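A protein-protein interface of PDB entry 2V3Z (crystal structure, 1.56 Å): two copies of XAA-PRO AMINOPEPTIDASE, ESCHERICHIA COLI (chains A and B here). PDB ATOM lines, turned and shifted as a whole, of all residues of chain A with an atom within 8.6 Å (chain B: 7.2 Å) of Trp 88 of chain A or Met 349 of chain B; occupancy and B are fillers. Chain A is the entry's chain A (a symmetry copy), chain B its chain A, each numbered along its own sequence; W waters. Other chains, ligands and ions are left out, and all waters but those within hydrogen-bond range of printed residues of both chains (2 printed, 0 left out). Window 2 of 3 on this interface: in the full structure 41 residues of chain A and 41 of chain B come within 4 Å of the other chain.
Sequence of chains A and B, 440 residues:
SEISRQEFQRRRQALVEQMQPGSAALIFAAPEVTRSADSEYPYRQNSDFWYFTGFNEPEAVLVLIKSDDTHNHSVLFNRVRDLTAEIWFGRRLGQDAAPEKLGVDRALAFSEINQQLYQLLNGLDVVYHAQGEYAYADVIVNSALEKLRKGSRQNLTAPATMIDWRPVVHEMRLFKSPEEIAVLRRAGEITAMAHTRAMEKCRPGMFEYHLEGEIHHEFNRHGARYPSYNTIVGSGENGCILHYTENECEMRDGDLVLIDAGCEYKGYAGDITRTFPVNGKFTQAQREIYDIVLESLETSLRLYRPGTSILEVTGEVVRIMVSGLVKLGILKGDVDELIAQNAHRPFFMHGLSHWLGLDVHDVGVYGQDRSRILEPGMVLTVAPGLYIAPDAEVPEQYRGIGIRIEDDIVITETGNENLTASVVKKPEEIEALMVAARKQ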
ATOM      1  N   ASP A  82      38.802 -18.709  14.364  1.00  0.00           N
ATOM      2  CA  ASP A  82      38.980 -17.810  13.217  1.00  0.00           C
ATOM      3  C   ASP A  82      37.955 -16.696  13.359  1.00  0.00           C
ATOM      4  O   ASP A  82      36.760 -16.935  13.198  1.00  0.00           O
ATOM      5  CB  ASP A  82      38.763 -18.596  11.917  1.00  0.00           C
ATOM      6  CG  ASP A  82      39.007 -17.782  10.658  1.00  0.00           C
ATOM      7  OD1 ASP A  82      38.408 -16.701  10.461  1.00  0.00           O
ATOM      8  OD2 ASP A  82      39.799 -18.261   9.822  1.00  0.00           O
ATOM      9  N   LEU A  83      38.415 -15.486  13.662  1.00  0.00           N
ATOM     10  CA  LEU A  83      37.495 -14.390  13.991  1.00  0.00           C
ATOM     11  C   LEU A  83      36.500 -14.130  12.875  1.00  0.00           C
ATOM     12  O   LEU A  83      35.301 -14.038  13.133  1.00  0.00           O
ATOM     13  CB  LEU A  83      38.261 -13.107  14.339  1.00  0.00           C
ATOM     14  CG  LEU A  83      37.416 -11.890  14.747  1.00  0.00           C
ATOM     15  CD1 LEU A  83      36.333 -12.274  15.764  1.00  0.00           C
ATOM     16  CD2 LEU A  83      38.313 -10.777  15.289  1.00  0.00           C
ATOM     17  N   THR A  84      36.982 -14.024  11.642  1.00  0.00           N
ATOM     18  CA  THR A  84      36.082 -13.712  10.519  1.00  0.00           C
ATOM     19  C   THR A  84      35.077 -14.817  10.250  1.00  0.00           C
ATOM     20  O   THR A  84      33.884 -14.561  10.053  1.00  0.00           O
ATOM     21  CB  THR A  84      36.862 -13.424   9.231  1.00  0.00           C
ATOM     22  OG1 THR A  84      37.688 -12.281   9.450  1.00  0.00           O
ATOM     23  CG2 THR A  84      35.896 -13.109   8.074  1.00  0.00           C
ATOM     24  N   ALA A  85      35.541 -16.054  10.243  1.00  0.00           N
ATOM     25  CA  ALA A  85      34.652 -17.174   9.991  1.00  0.00           C
ATOM     26  C   ALA A  85      33.598 -17.275  11.081  1.00  0.00           C
ATOM     27  O   ALA A  85      32.447 -17.645  10.819  1.00  0.00           O
ATOM     28  CB  ALA A  85      35.442 -18.496   9.876  1.00  0.00           C
ATOM     29  N   GLU A  86      33.984 -16.947  12.308  1.00  0.00           N
ATOM     30  CA  GLU A  86      33.053 -17.075  13.414  1.00  0.00           C
ATOM     31  C   GLU A  86      32.032 -15.934  13.427  1.00  0.00           C
ATOM     32  O   GLU A  86      30.859 -16.194  13.713  1.00  0.00           O
ATOM     33  CB  GLU A  86      33.794 -17.216  14.745  1.00  0.00           C
ATOM     34  CG  GLU A  86      34.570 -18.526  14.813  1.00  0.00           C
ATOM     35  CD  GLU A  86      35.238 -18.737  16.146  1.00  0.00           C
ATOM     36  OE1 GLU A  86      34.533 -18.731  17.180  1.00  0.00           O
ATOM     37  OE2 GLU A  86      36.471 -18.949  16.155  1.00  0.00           O
ATOM     38  N   ILE A  87      32.445 -14.703  13.116  1.00  0.00           N
ATOM     39  CA  ILE A  87      31.504 -13.565  12.946  1.00  0.00           C
ATOM     40  C   ILE A  87      30.436 -13.912  11.921  1.00  0.00           C
ATOM     41  O   ILE A  87      29.269 -13.531  12.061  1.00  0.00           O
ATOM     42  CB  ILE A  87      32.234 -12.273  12.480  1.00  0.00           C
ATOM     43  CG1 ILE A  87      33.029 -11.696  13.654  1.00  0.00           C
ATOM     44  CG2 ILE A  87      31.249 -11.215  11.890  1.00  0.00           C
ATOM     45  CD1 ILE A  87      34.003 -10.609  13.249  1.00  0.00           C
ATOM     46  N   TRP A  88      30.837 -14.591  10.861  1.00  0.00           N
ATOM     47  CA  TRP A  88      29.879 -14.951   9.815  1.00  0.00           C
ATOM     48  C   TRP A  88      29.050 -16.165  10.159  1.00  0.00           C
ATOM     49  O   TRP A  88      27.830 -16.128   9.997  1.00  0.00           O
ATOM     50  CB  TRP A  88      30.613 -15.176   8.492  1.00  0.00           C
ATOM     51  CG  TRP A  88      30.832 -13.909   7.776  1.00  0.00           C
ATOM     52  CD1 TRP A  88      31.843 -13.010   7.956  1.00  0.00           C
ATOM     53  CD2 TRP A  88      29.972 -13.347   6.775  1.00  0.00           C
ATOM     54  NE1 TRP A  88      31.677 -11.944   7.124  1.00  0.00           N
ATOM     55  CE2 TRP A  88      30.535 -12.124   6.383  1.00  0.00           C
ATOM     56  CE3 TRP A  88      28.785 -13.765   6.170  1.00  0.00           C
ATOM     57  CZ2 TRP A  88      29.955 -11.308   5.407  1.00  0.00           C
ATOM     58  CZ3 TRP A  88      28.208 -12.951   5.204  1.00  0.00           C
ATOM     59  CH2 TRP A  88      28.798 -11.749   4.835  1.00  0.00           C
ATOM     60  N   PHE A  89      29.697 -17.253  10.568  1.00  0.00           N
ATOM     61  CA  PHE A  89      29.039 -18.558  10.510  1.00  0.00           C
ATOM     62  C   PHE A  89      28.786 -19.233  11.832  1.00  0.00           C
ATOM     63  O   PHE A  89      28.029 -20.217  11.886  1.00  0.00           O
ATOM     64  CB  PHE A  89      29.821 -19.468   9.564  1.00  0.00           C
ATOM     65  CG  PHE A  89      29.984 -18.889   8.192  1.00  0.00           C
ATOM     66  CD1 PHE A  89      28.869 -18.553   7.432  1.00  0.00           C
ATOM     67  CD2 PHE A  89      31.231 -18.652   7.662  1.00  0.00           C
ATOM     68  CE1 PHE A  89      29.004 -18.003   6.180  1.00  0.00           C
ATOM     69  CE2 PHE A  89      31.374 -18.100   6.402  1.00  0.00           C
ATOM     70  CZ  PHE A  89      30.272 -17.785   5.656  1.00  0.00           C
ATOM     71  N   GLY A  90      29.381 -18.721  12.903  1.00  0.00           N
ATOM     72  CA  GLY A  90      29.126 -19.267  14.220  1.00  0.00           C
ATOM     73  C   GLY A  90      30.394 -19.573  14.971  1.00  0.00           C
ATOM     74  O   GLY A  90      31.460 -19.759  14.387  1.00  0.00           O
ATOM     75  N   ARG A  91      30.259 -19.695  16.280  1.00  0.00           N
ATOM     76  CA  ARG A  91      31.400 -19.946  17.136  1.00  0.00           C
ATOM     77  C   ARG A  91      31.964 -21.336  16.880  1.00  0.00           C
ATOM     78  O   ARG A  91      31.241 -22.271  16.512  1.00  0.00           O
ATOM     79  CB  ARG A  91      30.981 -19.832  18.597  1.00  0.00           C
ATOM     80  CG  ARG A  91      30.426 -18.463  18.980  1.00  0.00           C
ATOM     81  CD  ARG A  91      30.190 -18.349  20.464  1.00  0.00           C
ATOM     82  NE  ARG A  91      29.666 -17.032  20.790  1.00  0.00           N
ATOM     83  CZ  ARG A  91      28.370 -16.705  20.736  1.00  0.00           C
ATOM     84  NH1 ARG A  91      27.451 -17.610  20.404  1.00  0.00           N
ATOM     85  NH2 ARG A  91      28.004 -15.468  21.045  1.00  0.00           N
ATOM     86  N   ILE B 232      17.691 -17.875  11.575  1.00  0.00           N
ATOM     87  CA  ILE B 232      18.621 -17.242  12.516  1.00  0.00           C
ATOM     88  C   ILE B 232      17.822 -16.528  13.612  1.00  0.00           C
ATOM     89  O   ILE B 232      16.971 -15.686  13.300  1.00  0.00           O
ATOM     90  CB  ILE B 232      19.455 -16.196  11.730  1.00  0.00           C
ATOM     91  CG1 ILE B 232      20.371 -16.903  10.726  1.00  0.00           C
ATOM     92  CG2 ILE B 232      20.230 -15.250  12.637  1.00  0.00           C
ATOM     93  CD1 ILE B 232      20.705 -16.082   9.463  1.00  0.00           C
ATOM     94  N   CYS B 240      25.314 -10.519  16.828  1.00  0.00           N
ATOM     95  CA  CYS B 240      26.508 -10.078  16.120  1.00  0.00           C
ATOM     96  C   CYS B 240      27.131 -11.162  15.227  1.00  0.00           C
ATOM     97  O   CYS B 240      28.147 -10.920  14.578  1.00  0.00           O
ATOM     98  CB  CYS B 240      27.552  -9.617  17.110  1.00  0.00           C
ATOM     99  SG  CYS B 240      27.004  -8.185  18.080  1.00  0.00           S
ATOM    100  N   ILE B 241      26.554 -12.357  15.227  1.00  0.00           N
ATOM    101  CA  ILE B 241      26.983 -13.454  14.361  1.00  0.00           C
ATOM    102  C   ILE B 241      25.979 -13.514  13.216  1.00  0.00           C
ATOM    103  O   ILE B 241      24.772 -13.724  13.421  1.00  0.00           O
ATOM    104  CB  ILE B 241      27.019 -14.787  15.145  1.00  0.00           C
ATOM    105  CG1 ILE B 241      28.050 -14.713  16.278  1.00  0.00           C
ATOM    106  CG2 ILE B 241      27.311 -15.983  14.185  1.00  0.00           C
ATOM    107  CD1 ILE B 241      28.037 -15.930  17.238  1.00  0.00           C
ATOM    108  N   LEU B 242      26.458 -13.277  11.998  1.00  0.00           N
ATOM    109  CA  LEU B 242      25.575 -12.959  10.895  1.00  0.00           C
ATOM    110  C   LEU B 242      24.640 -14.091  10.506  1.00  0.00           C
ATOM    111  O   LEU B 242      23.463 -13.845  10.175  1.00  0.00           O
ATOM    112  CB  LEU B 242      26.374 -12.506   9.665  1.00  0.00           C
ATOM    113  CG  LEU B 242      27.226 -11.273   9.916  1.00  0.00           C
ATOM    114  CD1 LEU B 242      27.966 -10.887   8.622  1.00  0.00           C
ATOM    115  CD2 LEU B 242      26.397 -10.074  10.437  1.00  0.00           C
ATOM    116  N   HIS B 243      25.163 -15.314  10.496  1.00  0.00           N
ATOM    117  CA  HIS B 243      24.362 -16.515  10.154  1.00  0.00           C
ATOM    118  C   HIS B 243      24.217 -17.419  11.374  1.00  0.00           C
ATOM    119  O   HIS B 243      24.288 -18.645  11.271  1.00  0.00           O
ATOM    120  CB  HIS B 243      24.988 -17.329   9.010  1.00  0.00           C
ATOM    121  CG  HIS B 243      25.074 -16.624   7.696  1.00  0.00           C
ATOM    122  ND1 HIS B 243      25.466 -17.280   6.542  1.00  0.00           N
ATOM    123  CD2 HIS B 243      24.835 -15.344   7.334  1.00  0.00           C
ATOM    124  CE1 HIS B 243      25.467 -16.427   5.531  1.00  0.00           C
ATOM    125  NE2 HIS B 243      25.088 -15.247   5.982  1.00  0.00           N
ATOM    126  N   TYR B 244      24.006 -16.831  12.542  1.00  0.00           N
ATOM    127  CA  TYR B 244      23.838 -17.605  13.770  1.00  0.00           C
ATOM    128  C   TYR B 244      22.626 -18.511  13.699  1.00  0.00           C
ATOM    129  O   TYR B 244      21.501 -18.032  13.616  1.00  0.00           O
ATOM    130  CB  TYR B 244      23.685 -16.652  14.949  1.00  0.00           C
ATOM    131  CG  TYR B 244      23.375 -17.317  16.270  1.00  0.00           C
ATOM    132  CD1 TYR B 244      24.377 -17.914  17.036  1.00  0.00           C
ATOM    133  CD2 TYR B 244      22.085 -17.349  16.759  1.00  0.00           C
ATOM    134  CE1 TYR B 244      24.102 -18.531  18.251  1.00  0.00           C
ATOM    135  CE2 TYR B 244      21.800 -17.959  17.970  1.00  0.00           C
ATOM    136  CZ  TYR B 244      22.821 -18.551  18.723  1.00  0.00           C
ATOM    137  OH  TYR B 244      22.549 -19.148  19.930  1.00  0.00           O
ATOM    138  N   HIS B 344      33.361   2.301   8.605  1.00  0.00           N
ATOM    139  CA  HIS B 344      32.147   1.580   9.011  1.00  0.00           C
ATOM    140  C   HIS B 344      32.325   0.070   9.029  1.00  0.00           C
ATOM    141  O   HIS B 344      31.516  -0.626   9.646  1.00  0.00           O
ATOM    142  CB  HIS B 344      30.993   1.894   8.049  1.00  0.00           C
ATOM    143  CG  HIS B 344      31.245   1.424   6.656  1.00  0.00           C
ATOM    144  ND1 HIS B 344      32.211   1.987   5.853  1.00  0.00           N
ATOM    145  CD2 HIS B 344      30.686   0.427   5.931  1.00  0.00           C
ATOM    146  CE1 HIS B 344      32.228   1.364   4.691  1.00  0.00           C
ATOM    147  NE2 HIS B 344      31.324   0.400   4.716  1.00  0.00           N
ATOM    148  N   ARG B 345      33.361  -0.444   8.364  1.00  0.00           N
ATOM    149  CA  ARG B 345      33.467  -1.890   8.094  1.00  0.00           C
ATOM    150  C   ARG B 345      33.531  -2.807   9.319  1.00  0.00           C
ATOM    151  O   ARG B 345      33.030  -3.935   9.273  1.00  0.00           O
ATOM    152  CB  ARG B 345      34.641  -2.182   7.157  1.00  0.00           C
ATOM    153  CG  ARG B 345      34.310  -1.932   5.700  1.00  0.00           C
ATOM    154  CD  ARG B 345      35.480  -2.292   4.809  1.00  0.00           C
ATOM    155  NE  ARG B 345      35.135  -2.238   3.389  1.00  0.00           N
ATOM    156  CZ  ARG B 345      36.021  -2.182   2.396  1.00  0.00           C
ATOM    157  NH1 ARG B 345      37.329  -2.168   2.648  1.00  0.00           N
ATOM    158  NH2 ARG B 345      35.598  -2.139   1.138  1.00  0.00           N
ATOM    159  N   PRO B 346      34.139  -2.347  10.418  1.00  0.00           N
ATOM    160  CA  PRO B 346      34.076  -3.197  11.611  1.00  0.00           C
ATOM    161  C   PRO B 346      32.665  -3.431  12.137  1.00  0.00           C
ATOM    162  O   PRO B 346      32.444  -4.395  12.874  1.00  0.00           O
ATOM    163  CB  PRO B 346      34.879  -2.420  12.648  1.00  0.00           C
ATOM    164  CG  PRO B 346      35.781  -1.550  11.844  1.00  0.00           C
ATOM    165  CD  PRO B 346      34.978  -1.153  10.652  1.00  0.00           C
ATOM    166  N   PHE B 347      31.729  -2.556  11.757  1.00  0.00           N
ATOM    167  CA  PHE B 347      30.357  -2.606  12.259  1.00  0.00           C
ATOM    168  C   PHE B 347      29.309  -3.000  11.229  1.00  0.00           C
ATOM    169  O   PHE B 347      28.237  -3.467  11.598  1.00  0.00           O
ATOM    170  CB  PHE B 347      30.012  -1.235  12.850  1.00  0.00           C
ATOM    171  CG  PHE B 347      31.027  -0.750  13.828  1.00  0.00           C
ATOM    172  CD1 PHE B 347      31.205  -1.417  15.040  1.00  0.00           C
ATOM    173  CD2 PHE B 347      31.856   0.313  13.522  1.00  0.00           C
ATOM    174  CE1 PHE B 347      32.168  -0.996  15.951  1.00  0.00           C
ATOM    175  CE2 PHE B 347      32.822   0.747  14.427  1.00  0.00           C
ATOM    176  CZ  PHE B 347      32.980   0.098  15.636  1.00  0.00           C
ATOM    177  N   PHE B 348      29.615  -2.821   9.949  1.00  0.00           N
ATOM    178  CA  PHE B 348      28.730  -3.220   8.851  1.00  0.00           C
ATOM    179  C   PHE B 348      29.615  -3.885   7.816  1.00  0.00           C
ATOM    180  O   PHE B 348      30.250  -3.203   6.998  1.00  0.00           O
ATOM    181  CB  PHE B 348      27.969  -2.024   8.261  1.00  0.00           C
ATOM    182  CG  PHE B 348      27.126  -2.347   7.038  1.00  0.00           C
ATOM    183  CD1 PHE B 348      26.182  -3.367   7.063  1.00  0.00           C
ATOM    184  CD2 PHE B 348      27.230  -1.568   5.879  1.00  0.00           C
ATOM    185  CE1 PHE B 348      25.394  -3.617   5.959  1.00  0.00           C
ATOM    186  CE2 PHE B 348      26.446  -1.827   4.774  1.00  0.00           C
ATOM    187  CZ  PHE B 348      25.535  -2.846   4.820  1.00  0.00           C
ATOM    188  N   MET B 349      29.715  -5.212   7.909  1.00  0.00           N
ATOM    189  CA  MET B 349      30.741  -5.964   7.179  1.00  0.00           C
ATOM    190  C   MET B 349      30.193  -6.865   6.106  1.00  0.00           C
ATOM    191  O   MET B 349      30.905  -7.756   5.602  1.00  0.00           O
ATOM    192  CB  MET B 349      31.597  -6.780   8.147  1.00  0.00           C
ATOM    193  CG  MET B 349      30.899  -7.948   8.854  1.00  0.00           C
ATOM    194  SD  MET B 349      29.632  -7.468  10.059  1.00  0.00           S
ATOM    195  CE  MET B 349      30.592  -6.547  11.262  1.00  0.00           C
ATOM    196  N   HIS B 350      28.937  -6.660   5.743  1.00  0.00           N
ATOM    197  CA  HIS B 350      28.325  -7.392   4.662  1.00  0.00           C
ATOM    198  C   HIS B 350      27.667  -6.451   3.648  1.00  0.00           C
ATOM    199  O   HIS B 350      27.682  -5.230   3.819  1.00  0.00           O
ATOM    200  CB  HIS B 350      27.334  -8.428   5.194  1.00  0.00           C
ATOM    201  CG  HIS B 350      26.183  -7.854   5.981  1.00  0.00           C
ATOM    202  ND1 HIS B 350      25.061  -7.312   5.374  1.00  0.00           N
ATOM    203  CD2 HIS B 350      25.950  -7.814   7.317  1.00  0.00           C
ATOM    204  CE1 HIS B 350      24.197  -6.957   6.316  1.00  0.00           C
ATOM    205  NE2 HIS B 350      24.720  -7.230   7.498  1.00  0.00           N
ATOM    206  N   GLY B 351      27.190  -7.035   2.559  1.00  0.00           N
ATOM    207  CA  GLY B 351      26.528  -6.276   1.517  1.00  0.00           C
ATOM    208  C   GLY B 351      25.143  -5.830   1.915  1.00  0.00           C
ATOM    209  O   GLY B 351      24.486  -6.468   2.737  1.00  0.00           O
ATOM    210  N   HIS B 361      19.950 -16.497  -2.006  1.00  0.00           N
ATOM    211  CA  HIS B 361      21.018 -15.740  -2.667  1.00  0.00           C
ATOM    212  C   HIS B 361      20.912 -16.077  -4.153  1.00  0.00           C
ATOM    213  O   HIS B 361      21.507 -17.040  -4.652  1.00  0.00           O
ATOM    214  CB  HIS B 361      22.386 -16.098  -2.125  1.00  0.00           C
ATOM    215  CG  HIS B 361      22.588 -15.648  -0.718  1.00  0.00           C
ATOM    216  ND1 HIS B 361      23.591 -16.160   0.077  1.00  0.00           N
ATOM    217  CD2 HIS B 361      21.920 -14.757   0.036  1.00  0.00           C
ATOM    218  CE1 HIS B 361      23.527 -15.578   1.269  1.00  0.00           C
ATOM    219  NE2 HIS B 361      22.520 -14.723   1.273  1.00  0.00           N
ATOM    220  N   GLY B 385      22.720  -3.295   8.518  1.00  0.00           N
ATOM    221  CA  GLY B 385      22.863  -3.737   9.876  1.00  0.00           C
ATOM    222  C   GLY B 385      24.051  -3.068  10.522  1.00  0.00           C
ATOM    223  O   GLY B 385      24.926  -2.540   9.826  1.00  0.00           O
ATOM    224  N   LEU B 386      24.043  -3.073  11.850  1.00  0.00           N
ATOM    225  CA  LEU B 386      25.192  -2.651  12.648  1.00  0.00           C
ATOM    226  C   LEU B 386      25.407  -3.658  13.753  1.00  0.00           C
ATOM    227  O   LEU B 386      24.452  -4.065  14.427  1.00  0.00           O
ATOM    228  CB  LEU B 386      24.971  -1.255  13.227  1.00  0.00           C
ATOM    229  CG  LEU B 386      25.089  -0.107  12.231  1.00  0.00           C
ATOM    230  CD1 LEU B 386      24.586   1.201  12.879  1.00  0.00           C
ATOM    231  CD2 LEU B 386      26.518   0.073  11.665  1.00  0.00           C
ATOM    232  N   TYR B 387      26.660  -4.073  13.928  1.00  0.00           N
ATOM    233  CA  TYR B 387      27.016  -5.123  14.860  1.00  0.00           C
ATOM    234  C   TYR B 387      28.193  -4.647  15.666  1.00  0.00           C
ATOM    235  O   TYR B 387      29.266  -4.440  15.115  1.00  0.00           O
ATOM    236  CB  TYR B 387      27.339  -6.422  14.119  1.00  0.00           C
ATOM    237  CG  TYR B 387      26.349  -6.703  13.012  1.00  0.00           C
ATOM    238  CD1 TYR B 387      26.618  -6.298  11.709  1.00  0.00           C
ATOM    239  CD2 TYR B 387      25.144  -7.329  13.254  1.00  0.00           C
ATOM    240  CE1 TYR B 387      25.706  -6.505  10.685  1.00  0.00           C
ATOM    241  CE2 TYR B 387      24.228  -7.526  12.232  1.00  0.00           C
ATOM    242  CZ  TYR B 387      24.518  -7.115  10.947  1.00  0.00           C
ATOM    243  OH  TYR B 387      23.625  -7.331   9.925  1.00  0.00           O
ATOM    244  N   ILE B 388      27.962  -4.418  16.955  1.00  0.00           N
ATOM    245  CA  ILE B 388      28.968  -3.862  17.854  1.00  0.00           C
ATOM    246  C   ILE B 388      29.416  -4.987  18.766  1.00  0.00           C
ATOM    247  O   ILE B 388      28.682  -5.407  19.661  1.00  0.00           O
ATOM    248  CB  ILE B 388      28.429  -2.692  18.709  1.00  0.00           C
ATOM    249  CG1 ILE B 388      27.586  -1.682  17.895  1.00  0.00           C
ATOM    250  CG2 ILE B 388      29.600  -2.031  19.454  1.00  0.00           C
ATOM    251  CD1 ILE B 388      28.280  -1.014  16.761  1.00  0.00           C
HETATM  252  O   HOH W   1      33.061  -9.423   6.199  1.00  0.00           O
HETATM  253  O   HOH W   2      25.589 -20.898  13.454  1.00  0.00           O
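Water W1 lies within hydrogen-bond range of O of Met 349 of chain B (2.8 Å) and NE1 of Trp 88 of chain A (3.0 Å).
Water W2 bridges O of Phe 89 of chain A (3.0 Å) and O of His 243 of chain B (3.4 Å).
No position is printed for both chains.
Of the 11 pairs that touch across the chains among the printed residues, none has its exchanged pair printed and touching as well.
The side-chain sulfur (SG) of Cys 240 of chain B sits at hydrogen-bond distance from the backbone carbonyl oxygen (O) of Ile 388 of chain B, 3.6 Å away.
NE2 of His 350 of chain B sits at hydrogen-bond distance from OH of Tyr 387 of chain B (2.7 Å).
The side-chain carboxylate (OE2) of Glu 86 of chain A sits at hydrogen-bond distance from the backbone NH (N) of Asp 82 of chain A (2.9 Å).
Among the printed residues, pairs that only touch across the chains: Glu 86 of chain A with Ile 241 of chain B, Ile 87 of chain A with Cys 240 of chain B, Ile 87 of chain A with Ile 241 of chain B, Trp 88 of chain A with Leu 242 of chain B, Trp 88 of chain A with Met 349 of chain B, Trp 88 of chain A with His 350 of chain B, Phe 89 of chain A with His 243 of chain B, Gly 90 of chain A with Ile 241 of chain B and Arg 91 of chain A with Ile 241 of chain B.
Of the 19 printed residues of chain B, 6 touch a printed residue of chain A.
Hydrophobic or aromatic side chains of chain B that line the printed part of chain A: Ile 241, Leu 242, His 243 and His 350.
Of the 10 printed residues of chain A, 6 touch a printed residue of chain B.
Among the printed residues, 11 pairs touch across the chains.
Among the printed residues, no Asp or Glu carboxylate lies within 4 Å of a Lys or Arg side-chain nitrogen of the other chain.
Trp 88 of chain A touches just these residues of chain B: Leu 242 (3.6 Å), His 243 (2.8 Å), Met 349 (3.7 Å) and His 350 (3.6 Å).
Of the printed residues of chain A, Met 349 of chain B touches Trp 88.
Of chain A, only Trp 88 and Phe 89 come within 4 Å of His 243 of chain B.
Of the printed residues of chain A, Cys 240 of chain B touches Ile 87 (3.8 Å).
Of the printed residues of chain B, Arg 91 of chain A touches Ile 241.
Printed residues of chain A within 4 Å of His 350 of chain B: Trp 88 (3.6 Å).
Printed residues of chain B within 4 Å of Phe 89 of chain A: His 243.
Of the printed residues of chain A, Ile 241 of chain B touches Glu 86 (3.6 Å), Ile 87 (3.2 Å), Gly 90 (3.7 Å) and Arg 91 (3.6 Å).
Ala 85 of chain A touches none of the printed residues of chain B.
Ile 232 of chain B touches none of the printed residues of chain A.
The nearest printed residue of chain B that does not touch Phe 89 of chain A is Ile 241 of chain B (4.3 Å).
O of Ile 87 of chain A sits at hydrogen-bond distance from N of Leu 242 of chain B, at 2.8 Å.
O of Trp 88 of chain A sits at hydrogen-bond distance from N of His 243 of chain B (2.8 Å).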
